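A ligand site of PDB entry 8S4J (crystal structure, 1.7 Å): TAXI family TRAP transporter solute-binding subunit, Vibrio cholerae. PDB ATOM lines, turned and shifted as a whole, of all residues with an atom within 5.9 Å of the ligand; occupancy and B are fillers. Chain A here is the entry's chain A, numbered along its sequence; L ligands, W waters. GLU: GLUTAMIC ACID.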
ATOM      1  N   THR A  10     -32.856  -3.347 -29.390  1.00  0.00           N
ATOM      2  CA  THR A  10     -32.960  -3.229 -27.936  1.00  0.00           C
ATOM      3  C   THR A  10     -32.436  -4.469 -27.199  1.00  0.00           C
ATOM      4  O   THR A  10     -31.218  -4.641 -27.079  1.00  0.00           O
ATOM      5  CB  THR A  10     -34.421  -2.934 -27.516  1.00  0.00           C
ATOM      6  OG1 THR A  10     -35.281  -3.996 -27.963  1.00  0.00           O
ATOM      7  CG2 THR A  10     -34.901  -1.630 -28.142  1.00  0.00           C
ATOM      8  N   GLY A  11     -33.317  -5.301 -26.682  1.00  0.00           N
ATOM      9  CA  GLY A  11     -32.924  -6.485 -25.944  1.00  0.00           C
ATOM     10  C   GLY A  11     -34.104  -7.436 -25.850  1.00  0.00           C
ATOM     11  O   GLY A  11     -35.027  -7.375 -26.659  1.00  0.00           O
ATOM     12  N   SER A  12     -34.055  -8.317 -24.853  1.00  0.00           N
ATOM     13  CA  SER A  12     -35.156  -9.263 -24.655  1.00  0.00           C
ATOM     14  C   SER A  12     -36.405  -8.529 -24.200  1.00  0.00           C
ATOM     15  O   SER A  12     -36.341  -7.467 -23.554  1.00  0.00           O
ATOM     16  CB  SER A  12     -34.747 -10.345 -23.664  1.00  0.00           C
ATOM     17  OG  SER A  12     -35.045 -11.655 -24.158  1.00  0.00           O
ATOM     18  N   GLY A  15     -36.765  -7.230 -20.500  1.00  0.00           N
ATOM     19  CA  GLY A  15     -35.795  -6.314 -19.951  1.00  0.00           C
ATOM     20  C   GLY A  15     -36.257  -4.872 -19.979  1.00  0.00           C
ATOM     21  O   GLY A  15     -37.461  -4.580 -20.068  1.00  0.00           O
ATOM     22  N   VAL A  16     -35.297  -3.945 -19.860  1.00  0.00           N
ATOM     23  CA  VAL A  16     -35.635  -2.521 -19.888  1.00  0.00           C
ATOM     24  C   VAL A  16     -35.368  -1.928 -21.267  1.00  0.00           C
ATOM     25  O   VAL A  16     -36.066  -1.000 -21.699  1.00  0.00           O
ATOM     26  CB  VAL A  16     -34.903  -1.748 -18.778  1.00  0.00           C
ATOM     27  CG1 VAL A  16     -35.242  -0.249 -18.822  1.00  0.00           C
ATOM     28  CG2 VAL A  16     -35.198  -2.352 -17.401  1.00  0.00           C
ATOM     29  N   TYR A  17     -34.366  -2.425 -21.989  1.00  0.00           N
ATOM     30  CA  TYR A  17     -34.077  -1.856 -23.302  1.00  0.00           C
ATOM     31  C   TYR A  17     -35.289  -1.879 -24.226  1.00  0.00           C
ATOM     32  O   TYR A  17     -35.560  -0.917 -24.949  1.00  0.00           O
ATOM     33  CB  TYR A  17     -32.957  -2.628 -23.987  1.00  0.00           C
ATOM     34  CG  TYR A  17     -31.560  -2.382 -23.507  1.00  0.00           C
ATOM     35  CD1 TYR A  17     -31.280  -1.707 -22.328  1.00  0.00           C
ATOM     36  CD2 TYR A  17     -30.507  -2.877 -24.262  1.00  0.00           C
ATOM     37  CE1 TYR A  17     -29.961  -1.507 -21.909  1.00  0.00           C
ATOM     38  CE2 TYR A  17     -29.191  -2.704 -23.859  1.00  0.00           C
ATOM     39  CZ  TYR A  17     -28.921  -2.019 -22.694  1.00  0.00           C
ATOM     40  OH  TYR A  17     -27.597  -1.901 -22.336  1.00  0.00           O
ATOM     41  N   TYR A  18     -35.993  -3.016 -24.272  1.00  0.00           N
ATOM     42  CA  TYR A  18     -37.136  -3.137 -25.171  1.00  0.00           C
ATOM     43  C   TYR A  18     -38.197  -2.059 -24.910  1.00  0.00           C
ATOM     44  O   TYR A  18     -38.544  -1.335 -25.857  1.00  0.00           O
ATOM     45  CB  TYR A  18     -37.708  -4.562 -25.076  1.00  0.00           C
ATOM     46  CG  TYR A  18     -38.878  -4.798 -26.007  1.00  0.00           C
ATOM     47  CD1 TYR A  18     -38.703  -4.815 -27.384  1.00  0.00           C
ATOM     48  CD2 TYR A  18     -40.158  -5.014 -25.492  1.00  0.00           C
ATOM     49  CE1 TYR A  18     -39.776  -5.029 -28.241  1.00  0.00           C
ATOM     50  CE2 TYR A  18     -41.230  -5.242 -26.346  1.00  0.00           C
ATOM     51  CZ  TYR A  18     -41.042  -5.246 -27.709  1.00  0.00           C
ATOM     52  OH  TYR A  18     -42.121  -5.469 -28.539  1.00  0.00           O
ATOM     53  N   GLY A  45     -30.701  -9.650 -29.294  1.00  0.00           N
ATOM     54  CA  GLY A  45     -29.860 -10.297 -28.292  1.00  0.00           C
ATOM     55  C   GLY A  45     -29.170  -9.359 -27.318  1.00  0.00           C
ATOM     56  O   GLY A  45     -28.627  -9.840 -26.321  1.00  0.00           O
ATOM     57  N   GLY A  46     -29.178  -8.047 -27.574  1.00  0.00           N
ATOM     58  CA  GLY A  46     -28.549  -7.112 -26.645  1.00  0.00           C
ATOM     59  C   GLY A  46     -27.410  -6.299 -27.250  1.00  0.00           C
ATOM     60  O   GLY A  46     -27.312  -6.183 -28.469  1.00  0.00           O
ATOM     61  N   SER A  47     -26.538  -5.759 -26.381  1.00  0.00           N
ATOM     62  CA  SER A  47     -25.586  -4.717 -26.773  1.00  0.00           C
ATOM     63  C   SER A  47     -24.708  -5.130 -27.923  1.00  0.00           C
ATOM     64  O   SER A  47     -24.434  -4.326 -28.815  1.00  0.00           O
ATOM     65  CB  SER A  47     -24.680  -4.342 -25.583  1.00  0.00           C
ATOM     66  OG  SER A  47     -25.373  -3.616 -24.577  1.00  0.00           O
ATOM     67  N   ILE A  48     -24.161  -6.353 -27.869  1.00  0.00           N
ATOM     68  CA  ILE A  48     -23.144  -6.739 -28.858  1.00  0.00           C
ATOM     69  C   ILE A  48     -23.780  -6.893 -30.230  1.00  0.00           C
ATOM     70  O   ILE A  48     -23.300  -6.341 -31.239  1.00  0.00           O
ATOM     71  CB  ILE A  48     -22.426  -8.021 -28.405  1.00  0.00           C
ATOM     72  CG1 ILE A  48     -21.858  -7.867 -26.988  1.00  0.00           C
ATOM     73  CG2 ILE A  48     -21.334  -8.398 -29.411  1.00  0.00           C
ATOM     74  CD1 ILE A  48     -20.954  -6.648 -26.810  1.00  0.00           C
ATOM     75  N   ILE A  63     -29.536   0.280 -28.368  1.00  0.00           N
ATOM     76  CA  ILE A  63     -29.275   0.547 -26.959  1.00  0.00           C
ATOM     77  C   ILE A  63     -28.135  -0.362 -26.532  1.00  0.00           C
ATOM     78  O   ILE A  63     -28.161  -1.574 -26.753  1.00  0.00           O
ATOM     79  CB  ILE A  63     -30.537   0.353 -26.109  1.00  0.00           C
ATOM     80  CG1 ILE A  63     -31.648   1.237 -26.710  1.00  0.00           C
ATOM     81  CG2 ILE A  63     -30.250   0.761 -24.675  1.00  0.00           C
ATOM     82  CD1 ILE A  63     -32.990   1.163 -25.987  1.00  0.00           C
ATOM     83  N   VAL A  64     -27.089   0.252 -25.979  1.00  0.00           N
ATOM     84  CA  VAL A  64     -25.794  -0.428 -25.803  1.00  0.00           C
ATOM     85  C   VAL A  64     -25.213   0.034 -24.473  1.00  0.00           C
ATOM     86  O   VAL A  64     -25.239   1.236 -24.169  1.00  0.00           O
ATOM     87  CB  VAL A  64     -24.851  -0.092 -26.980  1.00  0.00           C
ATOM     88  CG1 VAL A  64     -23.476  -0.672 -26.733  1.00  0.00           C
ATOM     89  CG2 VAL A  64     -25.409  -0.637 -28.298  1.00  0.00           C
ATOM     90  N   GLN A  65     -24.694  -0.903 -23.677  1.00  0.00           N
ATOM     91  CA  GLN A  65     -24.045  -0.545 -22.423  1.00  0.00           C
ATOM     92  C   GLN A  65     -22.839   0.364 -22.675  1.00  0.00           C
ATOM     93  O   GLN A  65     -22.190   0.287 -23.717  1.00  0.00           O
ATOM     94  CB  GLN A  65     -23.542  -1.796 -21.694  1.00  0.00           C
ATOM     95  CG  GLN A  65     -24.656  -2.773 -21.260  1.00  0.00           C
ATOM     96  CD  GLN A  65     -24.114  -4.117 -20.746  1.00  0.00           C
ATOM     97  OE1 GLN A  65     -24.881  -5.082 -20.605  1.00  0.00           O
ATOM     98  NE2 GLN A  65     -22.822  -4.177 -20.432  1.00  0.00           N
ATOM     99  N   TRP A  68     -19.706  -1.422 -23.743  1.00  0.00           N
ATOM    100  CA  TRP A  68     -19.653  -1.866 -25.139  1.00  0.00           C
ATOM    101  C   TRP A  68     -19.776  -0.710 -26.132  1.00  0.00           C
ATOM    102  O   TRP A  68     -19.365  -0.882 -27.289  1.00  0.00           O
ATOM    103  CB  TRP A  68     -20.701  -2.983 -25.358  1.00  0.00           C
ATOM    104  CG  TRP A  68     -20.406  -4.032 -24.323  1.00  0.00           C
ATOM    105  CD1 TRP A  68     -21.228  -4.498 -23.330  1.00  0.00           C
ATOM    106  CD2 TRP A  68     -19.128  -4.655 -24.096  1.00  0.00           C
ATOM    107  NE1 TRP A  68     -20.539  -5.387 -22.518  1.00  0.00           N
ATOM    108  CE2 TRP A  68     -19.248  -5.487 -22.980  1.00  0.00           C
ATOM    109  CE3 TRP A  68     -17.889  -4.590 -24.770  1.00  0.00           C
ATOM    110  CZ2 TRP A  68     -18.172  -6.234 -22.482  1.00  0.00           C
ATOM    111  CZ3 TRP A  68     -16.834  -5.335 -24.284  1.00  0.00           C
ATOM    112  CH2 TRP A  68     -16.987  -6.153 -23.164  1.00  0.00           C
ATOM    113  N   HIS A  95     -30.556   5.039 -18.072  1.00  0.00           N
ATOM    114  CA  HIS A  95     -30.521   4.499 -16.720  1.00  0.00           C
ATOM    115  C   HIS A  95     -29.261   3.681 -16.449  1.00  0.00           C
ATOM    116  O   HIS A  95     -28.549   3.247 -17.364  1.00  0.00           O
ATOM    117  CB  HIS A  95     -31.741   3.591 -16.486  1.00  0.00           C
ATOM    118  CG  HIS A  95     -31.855   2.515 -17.511  1.00  0.00           C
ATOM    119  ND1 HIS A  95     -32.293   2.763 -18.794  1.00  0.00           N
ATOM    120  CD2 HIS A  95     -31.559   1.192 -17.455  1.00  0.00           C
ATOM    121  CE1 HIS A  95     -32.266   1.635 -19.491  1.00  0.00           C
ATOM    122  NE2 HIS A  95     -31.827   0.677 -18.698  1.00  0.00           N
ATOM    123  N   GLU A  97     -27.374   0.300 -15.174  1.00  0.00           N
ATOM    124  CA  GLU A  97     -27.579  -1.150 -15.273  1.00  0.00           C
ATOM    125  C   GLU A  97     -26.587  -1.881 -14.374  1.00  0.00           C
ATOM    126  O   GLU A  97     -25.429  -2.103 -14.790  1.00  0.00           O
ATOM    127  CB  GLU A  97     -27.407  -1.637 -16.721  1.00  0.00           C
ATOM    128  CG  GLU A  97     -28.145  -0.831 -17.766  1.00  0.00           C
ATOM    129  CD  GLU A  97     -28.005  -1.497 -19.108  1.00  0.00           C
ATOM    130  OE1 GLU A  97     -28.655  -2.548 -19.314  1.00  0.00           O
ATOM    131  OE2 GLU A  97     -27.221  -1.001 -19.958  1.00  0.00           O
ATOM    132  N   ASN A 124     -26.435 -14.952 -23.447  1.00  0.00           N
ATOM    133  CA  ASN A 124     -26.447 -15.321 -24.843  1.00  0.00           C
ATOM    134  C   ASN A 124     -25.383 -14.534 -25.624  1.00  0.00           C
ATOM    135  O   ASN A 124     -25.003 -13.433 -25.218  1.00  0.00           O
ATOM    136  CB  ASN A 124     -27.827 -15.058 -25.457  1.00  0.00           C
ATOM    137  CG  ASN A 124     -28.292 -13.629 -25.271  1.00  0.00           C
ATOM    138  OD1 ASN A 124     -28.614 -13.207 -24.141  1.00  0.00           O
ATOM    139  ND2 ASN A 124     -28.346 -12.875 -26.352  1.00  0.00           N
ATOM    140  N   GLY A 126     -25.124 -12.622 -28.240  1.00  0.00           N
ATOM    141  CA  GLY A 126     -25.218 -11.216 -28.609  1.00  0.00           C
ATOM    142  C   GLY A 126     -25.378 -10.232 -27.464  1.00  0.00           C
ATOM    143  O   GLY A 126     -25.521  -9.038 -27.711  1.00  0.00           O
ATOM    144  N   SER A 127     -25.354 -10.682 -26.209  1.00  0.00           N
ATOM    145  CA  SER A 127     -25.742  -9.824 -25.109  1.00  0.00           C
ATOM    146  C   SER A 127     -24.564  -9.081 -24.471  1.00  0.00           C
ATOM    147  O   SER A 127     -23.442  -9.598 -24.401  1.00  0.00           O
ATOM    148  CB  SER A 127     -26.460 -10.630 -24.018  1.00  0.00           C
ATOM    149  OG  SER A 127     -25.590 -11.575 -23.408  1.00  0.00           O
ATOM    150  N   GLY A 128     -24.855  -7.871 -23.985  1.00  0.00           N
ATOM    151  CA  GLY A 128     -23.956  -7.229 -23.049  1.00  0.00           C
ATOM    152  C   GLY A 128     -23.767  -8.024 -21.782  1.00  0.00           C
ATOM    153  O   GLY A 128     -22.726  -7.935 -21.128  1.00  0.00           O
ATOM    154  N   ASP A 129     -24.784  -8.828 -21.418  1.00  0.00           N
ATOM    155  CA  ASP A 129     -24.674  -9.696 -20.259  1.00  0.00           C
ATOM    156  C   ASP A 129     -23.432 -10.576 -20.366  1.00  0.00           C
ATOM    157  O   ASP A 129     -22.595 -10.603 -19.462  1.00  0.00           O
ATOM    158  CB  ASP A 129     -25.908 -10.609 -20.144  1.00  0.00           C
ATOM    159  CG  ASP A 129     -27.224  -9.820 -20.133  1.00  0.00           C
ATOM    160  OD1 ASP A 129     -27.278  -8.709 -19.568  1.00  0.00           O
ATOM    161  OD2 ASP A 129     -28.232 -10.361 -20.649  1.00  0.00           O
ATOM    162  N   TYR A 172     -27.517 -10.795 -15.103  1.00  0.00           N
ATOM    163  CA  TYR A 172     -28.280  -9.926 -15.991  1.00  0.00           C
ATOM    164  C   TYR A 172     -27.783  -8.513 -15.767  1.00  0.00           C
ATOM    165  O   TYR A 172     -27.850  -7.986 -14.652  1.00  0.00           O
ATOM    166  CB  TYR A 172     -29.794 -10.018 -15.706  1.00  0.00           C
ATOM    167  CG  TYR A 172     -30.700  -9.835 -16.928  1.00  0.00           C
ATOM    168  CD1 TYR A 172     -30.311  -9.076 -18.010  1.00  0.00           C
ATOM    169  CD2 TYR A 172     -31.981 -10.394 -16.953  1.00  0.00           C
ATOM    170  CE1 TYR A 172     -31.150  -8.895 -19.127  1.00  0.00           C
ATOM    171  CE2 TYR A 172     -32.835 -10.224 -18.053  1.00  0.00           C
ATOM    172  CZ  TYR A 172     -32.416  -9.481 -19.126  1.00  0.00           C
ATOM    173  OH  TYR A 172     -33.260  -9.303 -20.199  1.00  0.00           O
ATOM    174  N   MET A 173     -27.265  -7.908 -16.835  1.00  0.00           N
ATOM    175  CA  MET A 173     -26.800  -6.527 -16.848  1.00  0.00           C
ATOM    176  C   MET A 173     -28.060  -5.729 -17.215  1.00  0.00           C
ATOM    177  O   MET A 173     -28.413  -5.643 -18.389  1.00  0.00           O
ATOM    178  CB  MET A 173     -25.761  -6.405 -17.945  1.00  0.00           C
ATOM    179  CG  MET A 173     -24.282  -6.586 -17.646  1.00  0.00           C
ATOM    180  SD  MET A 173     -23.510  -6.270 -16.074  1.00  0.00           S
ATOM    181  CE  MET A 173     -23.337  -4.536 -16.216  1.00  0.00           C
ATOM    182  N   VAL A 174     -28.799  -5.205 -16.234  1.00  0.00           N
ATOM    183  CA  VAL A 174     -30.117  -4.669 -16.549  1.00  0.00           C
ATOM    184  C   VAL A 174     -30.532  -3.673 -15.474  1.00  0.00           C
ATOM    185  O   VAL A 174     -30.149  -3.794 -14.303  1.00  0.00           O
ATOM    186  CB  VAL A 174     -31.157  -5.808 -16.720  1.00  0.00           C
ATOM    187  CG1 VAL A 174     -31.349  -6.579 -15.444  1.00  0.00           C
ATOM    188  CG2 VAL A 174     -32.492  -5.283 -17.253  1.00  0.00           C
ATOM    189  N   GLY A 175     -31.304  -2.664 -15.885  1.00  0.00           N
ATOM    190  CA  GLY A 175     -31.889  -1.709 -14.960  1.00  0.00           C
ATOM    191  C   GLY A 175     -33.052  -2.267 -14.149  1.00  0.00           C
ATOM    192  O   GLY A 175     -33.479  -3.417 -14.294  1.00  0.00           O
HETATM  193  N   GLU L   1     -27.595  -4.645 -21.009  1.00  0.00           N
HETATM  194  CA  GLU L   1     -28.211  -5.887 -21.535  1.00  0.00           C
HETATM  195  C   GLU L   1     -27.478  -6.311 -22.789  1.00  0.00           C
HETATM  196  O   GLU L   1     -27.568  -7.509 -23.180  1.00  0.00           O
HETATM  197  CB  GLU L   1     -29.671  -5.650 -21.933  1.00  0.00           C
HETATM  198  CG  GLU L   1     -30.474  -5.182 -20.712  1.00  0.00           C
HETATM  199  CD  GLU L   1     -31.951  -4.957 -21.065  1.00  0.00           C
HETATM  200  OE1 GLU L   1     -32.599  -4.036 -20.482  1.00  0.00           O
HETATM  201  OE2 GLU L   1     -32.503  -5.653 -21.951  1.00  0.00           O
HETATM  202  OXT GLU L   1     -26.807  -5.461 -23.416  1.00  0.00           O
HETATM  203  O   HOH W   1     -32.238  -8.234 -22.463  1.00  0.00           O
HETATM  204  O   HOH W   2     -29.668  -9.157 -22.546  1.00  0.00           O
HETATM  205  O   HOH W   3     -31.297  -2.205 -18.860  1.00  0.00           O
HETATM  206  O   HOH W   4     -34.954  -5.336 -23.017  1.00  0.00           O
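Water W1 lies within hydrogen-bond range of OE2 of the ligand (2.6 Å), OH of Tyr 172 (2.7 Å) and N of Ser 12 (3.0 Å).
Water W2 bridges OD2 of Asp 129 (2.7 Å) and O of the ligand (2.7 Å).
Water W3 lies within hydrogen-bond range of OE1 of Glu 97, OE1 of the ligand, NE2 of His 95 and N of Gly 175.
Gly 15 touches the ligand.
CA of Gly 46 touches O of the ligand, 3.6 Å away.
CB of Ser 127 touches O of the ligand (3.4 Å).
Asp 129 touches the ligand.
CG2 of Val 174 touches OE1 of the ligand, 3.5 Å away.
Hydrophobic or aromatic side chains that line the ligand: Val 16, Tyr 17, Met 173 and Val 174.
Of the 26 residues printed, 12 come within 4 Å of the ligand.
Along chain A the residues within 4 Å of the ligand span positions 15 to 174.
N of Ser 47 lies within hydrogen-bond range of OXT of the ligand (3.0 Å).
The side-chain hydroxyl of Ser 47 lies within hydrogen-bond range of an oxygen (OXT) of the ligand (2.6 Å).
N of Val 16 sits at hydrogen-bond distance from OE1 of the ligand (2.8 Å).
N of the ligand lies within hydrogen-bond range of OE1 of Gln 65, at 2.8 Å.
The backbone NH of Tyr 17 is in hydrogen-bond range of an oxygen (OE1) of the ligand, 2.8 Å away.
The side-chain hydroxyl (OH) of Tyr 17 lies within hydrogen-bond range of a nitrogen (N) of the ligand, 3.0 Å away.
The backbone NH (N) of Gly 128 lies within hydrogen-bond range of an oxygen (O) of the ligand.
OE1 of Glu 97 is in salt-bridge range of N of the ligand (2.9 Å).
The backbone carbonyl oxygen of Met 173 lies within hydrogen-bond range of a nitrogen (N) of the ligand (2.9 Å).
The side-chain hydroxyl (OG) of Ser 47 lies within hydrogen-bond range of the backbone NH (N) of Gln 65 (2.9 Å).
The backbone NH (N) of Gln 65 lies close to the side-chain hydroxyl (OH) of Tyr 17 (3.3 Å).
The indole nitrogen (NE1) of Trp 68 lies close to the side-chain amide nitrogen (NE2) of Gln 65, 3.3 Å away.
OH of Tyr 17 lies within hydrogen-bond range of OE2 of Glu 97 (2.6 Å).
The side-chain carboxylate (OD1) of Asp 129 is in hydrogen-bond range of the backbone NH (N) of Met 173 (2.8 Å).
The side-chain hydroxyl (OG) of Ser 127 lies close to the backbone NH (N) of Asp 129, at 3.5 Å.
N of Ser 127 sits close to O of Gly 45, at 3.4 Å.
The side-chain hydroxyl (OG) of Ser 127 is in hydrogen-bond range of the backbone carbonyl oxygen (O) of Asn 124 (2.7 Å).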
